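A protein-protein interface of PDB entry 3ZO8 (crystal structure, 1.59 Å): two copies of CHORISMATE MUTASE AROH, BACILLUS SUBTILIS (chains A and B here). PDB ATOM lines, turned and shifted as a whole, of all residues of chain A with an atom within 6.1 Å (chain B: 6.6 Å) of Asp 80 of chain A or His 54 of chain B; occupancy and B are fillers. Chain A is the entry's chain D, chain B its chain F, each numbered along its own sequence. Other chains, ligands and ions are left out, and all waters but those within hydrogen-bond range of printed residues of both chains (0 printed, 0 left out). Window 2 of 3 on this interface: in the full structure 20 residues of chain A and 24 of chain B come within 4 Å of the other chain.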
ATOM      1  N   PRO A  51      -0.292  -4.262  21.805  1.00  0.00           N
ATOM      2  CA  PRO A  51      -0.853  -3.632  20.588  1.00  0.00           C
ATOM      3  C   PRO A  51      -0.939  -4.526  19.338  1.00  0.00           C
ATOM      4  O   PRO A  51      -1.508  -4.112  18.327  1.00  0.00           O
ATOM      5  CB  PRO A  51       0.072  -2.427  20.345  1.00  0.00           C
ATOM      6  CG  PRO A  51       1.308  -2.716  21.123  1.00  0.00           C
ATOM      7  CD  PRO A  51       0.905  -3.560  22.294  1.00  0.00           C
ATOM      8  N   GLU A  78      -1.761  -2.193  26.630  1.00  0.00           N
ATOM      9  CA  GLU A  78      -0.491  -2.287  27.319  1.00  0.00           C
ATOM     10  C   GLU A  78       0.582  -1.492  26.570  1.00  0.00           C
ATOM     11  O   GLU A  78       0.541  -1.363  25.333  1.00  0.00           O
ATOM     12  CB  GLU A  78      -0.078  -3.756  27.480  1.00  0.00           C
ATOM     13  CG  GLU A  78       1.333  -4.001  28.008  1.00  0.00           C
ATOM     14  CD  GLU A  78       1.554  -3.498  29.424  1.00  0.00           C
ATOM     15  OE1 GLU A  78       1.722  -2.274  29.613  1.00  0.00           O
ATOM     16  OE2 GLU A  78       1.590  -4.328  30.354  1.00  0.00           O
ATOM     17  N   MET A  79       1.519  -0.942  27.337  1.00  0.00           N
ATOM     18  CA  MET A  79       2.717  -0.296  26.805  1.00  0.00           C
ATOM     19  C   MET A  79       3.439  -1.207  25.830  1.00  0.00           C
ATOM     20  O   MET A  79       3.529  -2.408  26.060  1.00  0.00           O
ATOM     21  CB  MET A  79       3.687   0.012  27.940  1.00  0.00           C
ATOM     22  CG  MET A  79       3.417   1.289  28.705  1.00  0.00           C
ATOM     23  SD  MET A  79       4.706   1.519  29.943  1.00  0.00           S
ATOM     24  CE  MET A  79       6.180   1.506  28.928  1.00  0.00           C
ATOM     25  N   ASP A  80       3.978  -0.624  24.759  1.00  0.00           N
ATOM     26  CA  ASP A  80       4.781  -1.360  23.781  1.00  0.00           C
ATOM     27  C   ASP A  80       6.262  -1.195  24.110  1.00  0.00           C
ATOM     28  O   ASP A  80       6.905  -0.249  23.642  1.00  0.00           O
ATOM     29  CB  ASP A  80       4.515  -0.823  22.374  1.00  0.00           C
ATOM     30  CG  ASP A  80       4.785  -1.851  21.286  1.00  0.00           C
ATOM     31  OD1 ASP A  80       5.365  -2.915  21.586  1.00  0.00           O
ATOM     32  OD2 ASP A  80       4.406  -1.589  20.120  1.00  0.00           O
ATOM     33  N   VAL A  81       6.801  -2.116  24.905  1.00  0.00           N
ATOM     34  CA  VAL A  81       8.187  -2.033  25.362  1.00  0.00           C
ATOM     35  C   VAL A  81       9.109  -2.863  24.496  1.00  0.00           C
ATOM     36  O   VAL A  81       8.754  -3.970  24.080  1.00  0.00           O
ATOM     37  CB  VAL A  81       8.333  -2.493  26.827  1.00  0.00           C
ATOM     38  CG1 VAL A  81       9.803  -2.636  27.212  1.00  0.00           C
ATOM     39  CG2 VAL A  81       7.616  -1.519  27.745  1.00  0.00           C
ATOM     40  N   THR A  82      10.295  -2.315  24.242  1.00  0.00           N
ATOM     41  CA  THR A  82      11.308  -2.958  23.413  1.00  0.00           C
ATOM     42  C   THR A  82      11.684  -4.330  23.980  1.00  0.00           C
ATOM     43  O   THR A  82      12.139  -4.441  25.121  1.00  0.00           O
ATOM     44  CB  THR A  82      12.550  -2.048  23.260  1.00  0.00           C
ATOM     45  OG1 THR A  82      12.148  -0.783  22.711  1.00  0.00           O
ATOM     46  CG2 THR A  82      13.580  -2.682  22.342  1.00  0.00           C
ATOM     47  N   GLY A  83      11.471  -5.380  23.186  1.00  0.00           N
ATOM     48  CA  GLY A  83      11.708  -6.751  23.645  1.00  0.00           C
ATOM     49  C   GLY A  83      10.603  -7.337  24.515  1.00  0.00           C
ATOM     50  O   GLY A  83      10.639  -8.521  24.863  1.00  0.00           O
ATOM     51  N   ASP B  15      14.684   8.368  26.456  1.00  0.00           N
ATOM     52  CA  ASP B  15      13.969   7.091  26.579  1.00  0.00           C
ATOM     53  C   ASP B  15      14.946   5.939  26.748  1.00  0.00           C
ATOM     54  O   ASP B  15      15.126   5.118  25.843  1.00  0.00           O
ATOM     55  CB  ASP B  15      13.066   6.835  25.364  1.00  0.00           C
ATOM     56  CG  ASP B  15      12.367   5.473  25.420  1.00  0.00           C
ATOM     57  OD1 ASP B  15      12.095   4.969  26.533  1.00  0.00           O
ATOM     58  OD2 ASP B  15      12.085   4.910  24.342  1.00  0.00           O
ATOM     59  N   ILE B  20      14.243   6.048  32.842  1.00  0.00           N
ATOM     60  CA  ILE B  20      12.874   5.687  33.189  1.00  0.00           C
ATOM     61  C   ILE B  20      12.816   5.091  34.607  1.00  0.00           C
ATOM     62  O   ILE B  20      12.031   5.549  35.434  1.00  0.00           O
ATOM     63  CB  ILE B  20      12.213   4.755  32.147  1.00  0.00           C
ATOM     64  CG1 ILE B  20      12.009   5.491  30.818  1.00  0.00           C
ATOM     65  CG2 ILE B  20      10.879   4.241  32.667  1.00  0.00           C
ATOM     66  CD1 ILE B  20      11.256   4.691  29.775  1.00  0.00           C
ATOM     67  N   THR B  50       3.619   7.753  28.094  1.00  0.00           N
ATOM     68  CA  THR B  50       3.339   8.245  26.741  1.00  0.00           C
ATOM     69  C   THR B  50       3.995   7.370  25.667  1.00  0.00           C
ATOM     70  O   THR B  50       4.967   6.667  25.932  1.00  0.00           O
ATOM     71  CB  THR B  50       3.776   9.703  26.594  1.00  0.00           C
ATOM     72  OG1 THR B  50       5.124   9.826  27.046  1.00  0.00           O
ATOM     73  CG2 THR B  50       2.890  10.602  27.467  1.00  0.00           C
ATOM     74  N   PRO B  51       3.462   7.410  24.438  1.00  0.00           N
ATOM     75  CA  PRO B  51       3.954   6.458  23.445  1.00  0.00           C
ATOM     76  C   PRO B  51       5.344   6.767  22.863  1.00  0.00           C
ATOM     77  O   PRO B  51       5.751   6.109  21.905  1.00  0.00           O
ATOM     78  CB  PRO B  51       2.870   6.477  22.357  1.00  0.00           C
ATOM     79  CG  PRO B  51       2.146   7.770  22.535  1.00  0.00           C
ATOM     80  CD  PRO B  51       2.326   8.217  23.957  1.00  0.00           C
ATOM     81  N   ASP B  52       6.061   7.735  23.433  1.00  0.00           N
ATOM     82  CA  ASP B  52       7.464   7.979  23.057  1.00  0.00           C
ATOM     83  C   ASP B  52       8.459   7.169  23.889  1.00  0.00           C
ATOM     84  O   ASP B  52       9.660   7.154  23.598  1.00  0.00           O
ATOM     85  CB  ASP B  52       7.831   9.477  23.075  1.00  0.00           C
ATOM     86  CG  ASP B  52       7.232  10.236  24.258  1.00  0.00           C
ATOM     87  OD1 ASP B  52       6.914   9.615  25.297  1.00  0.00           O
ATOM     88  OD2 ASP B  52       7.094  11.476  24.145  1.00  0.00           O
ATOM     89  N   LEU B  53       7.948   6.499  24.921  1.00  0.00           N
ATOM     90  CA  LEU B  53       8.767   5.691  25.833  1.00  0.00           C
ATOM     91  C   LEU B  53       8.585   4.184  25.621  1.00  0.00           C
ATOM     92  O   LEU B  53       7.504   3.637  25.850  1.00  0.00           O
ATOM     93  CB  LEU B  53       8.451   6.059  27.284  1.00  0.00           C
ATOM     94  CG  LEU B  53       8.479   7.568  27.545  1.00  0.00           C
ATOM     95  CD1 LEU B  53       7.875   7.927  28.896  1.00  0.00           C
ATOM     96  CD2 LEU B  53       9.896   8.116  27.403  1.00  0.00           C
ATOM     97  N   HIS B  54       9.647   3.511  25.193  1.00  0.00           N
ATOM     98  CA  HIS B  54       9.582   2.069  24.951  1.00  0.00           C
ATOM     99  C   HIS B  54      10.664   1.274  25.638  1.00  0.00           C
ATOM    100  O   HIS B  54      10.709   0.058  25.484  1.00  0.00           O
ATOM    101  CB  HIS B  54       9.645   1.765  23.451  1.00  0.00           C
ATOM    102  CG  HIS B  54       8.880   2.740  22.583  1.00  0.00           C
ATOM    103  ND1 HIS B  54       7.616   2.514  22.179  1.00  0.00           N
ATOM    104  CD2 HIS B  54       9.258   3.962  22.026  1.00  0.00           C
ATOM    105  CE1 HIS B  54       7.199   3.545  21.414  1.00  0.00           C
ATOM    106  NE2 HIS B  54       8.207   4.428  21.321  1.00  0.00           N
ATOM    107  N   ALA B  55      11.541   1.932  26.399  1.00  0.00           N
ATOM    108  CA  ALA B  55      12.771   1.287  26.908  1.00  0.00           C
ATOM    109  C   ALA B  55      12.558   0.184  27.948  1.00  0.00           C
ATOM    110  O   ALA B  55      13.301  -0.806  27.992  1.00  0.00           O
ATOM    111  CB  ALA B  55      13.738   2.333  27.445  1.00  0.00           C
ATOM    112  N   VAL B  56      11.553   0.367  28.790  1.00  0.00           N
ATOM    113  CA  VAL B  56      11.272  -0.566  29.869  1.00  0.00           C
ATOM    114  C   VAL B  56       9.881  -0.296  30.420  1.00  0.00           C
ATOM    115  O   VAL B  56       9.327   0.789  30.213  1.00  0.00           O
ATOM    116  CB  VAL B  56      12.316  -0.441  31.002  1.00  0.00           C
ATOM    117  CG1 VAL B  56      12.379   0.989  31.531  1.00  0.00           C
ATOM    118  CG2 VAL B  56      12.019  -1.432  32.120  1.00  0.00           C
ATOM    119  N   PHE B  57       9.305  -1.288  31.095  1.00  0.00           N
ATOM    120  CA  PHE B  57       8.109  -1.051  31.885  1.00  0.00           C
ATOM    121  C   PHE B  57       8.550  -0.318  33.135  1.00  0.00           C
ATOM    122  O   PHE B  57       9.453  -0.783  33.840  1.00  0.00           O
ATOM    123  CB  PHE B  57       7.427  -2.361  32.289  1.00  0.00           C
ATOM    124  CG  PHE B  57       6.716  -3.051  31.160  1.00  0.00           C
ATOM    125  CD1 PHE B  57       5.646  -2.443  30.517  1.00  0.00           C
ATOM    126  CD2 PHE B  57       7.107  -4.313  30.750  1.00  0.00           C
ATOM    127  CE1 PHE B  57       4.990  -3.083  29.481  1.00  0.00           C
ATOM    128  CE2 PHE B  57       6.453  -4.959  29.718  1.00  0.00           C
ATOM    129  CZ  PHE B  57       5.395  -4.343  29.081  1.00  0.00           C
ATOM    130  N   GLN B  77      -0.628   2.204  28.270  1.00  0.00           N
ATOM    131  CA  GLN B  77      -0.248   3.310  27.433  1.00  0.00           C
ATOM    132  C   GLN B  77      -1.165   4.502  27.707  1.00  0.00           C
ATOM    133  O   GLN B  77      -2.379   4.341  27.799  1.00  0.00           O
ATOM    134  CB  GLN B  77      -0.357   2.883  25.981  1.00  0.00           C
ATOM    135  CG  GLN B  77       0.007   3.962  24.989  1.00  0.00           C
ATOM    136  CD  GLN B  77       0.005   3.426  23.577  1.00  0.00           C
ATOM    137  OE1 GLN B  77      -1.048   3.098  23.025  1.00  0.00           O
ATOM    138  NE2 GLN B  77       1.185   3.307  22.993  1.00  0.00           N
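O of Asp 80 of chain A sits at hydrogen-bond distance from ND1 of His 54 of chain B. N of Thr 82 of chain A sits at hydrogen-bond distance from O of His 54 of chain B.
N of His 54 of chain B is in hydrogen-bond range of OD2 of Asp 15 of chain B (2.9 Å). A ring nitrogen (NE2) of His 54 of chain B sits close to the backbone carbonyl oxygen of Pro 51 of chain B.
Among the printed residues, pairs that only touch across the chains: Val 81 of chain A with His 54 of chain B (3.3 Å), Glu 78 of chain A with Phe 57 of chain B (3.4 Å), Met 79 of chain A with Val 56 of chain B (3.5 Å), Val 81 of chain A with Phe 57 of chain B (3.5 Å), Val 81 of chain A with Val 56 of chain B (3.7 Å), Met 79 of chain A with Phe 57 of chain B (3.7 Å), Met 79 of chain A with Gln 77 of chain B (3.9 Å) and Met 79 of chain A with Leu 53 of chain B (3.97 Å).
Printed residues of chain B within 4 Å of Asp 80 of chain A: His 54. His 54 of chain B touches just these residues of chain A: Asp 80 (3.2 Å), Val 81 (3.3 Å) and Thr 82 (2.7 Å). Of the printed residues of chain A, Val 56 of chain B touches Met 79 and Val 81. Printed residues of chain A within 4 Å of Leu 53 of chain B: Met 79. Printed residues of chain B within 4 Å of Thr 82 of chain A: His 54. Pro 51 of chain B touches none of the printed residues of chain A. Asp 15 of chain B touches none of the printed residues of chain A. The nearest residue of chain B that does not touch Asp 80 of chain A is Leu 53 of chain B (4.5 Å).
Printed residues of chain A that touch a printed residue of chain B: Glu 78, Met 79, Asp 80, Val 81 and Thr 82. Hydrophobic or aromatic side chains of chain A that line the printed part of chain B: Met 79 and Val 81. Along chain A the printed residues that touch a printed residue of chain B span positions 78 to 82. Among the printed residues, 10 pairs touch across the chains. Among the printed residues, no Asp or Glu carboxylate lies within 4 Å of a Lys or Arg side-chain nitrogen of the other chain.
Position printed for both chains: 51.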
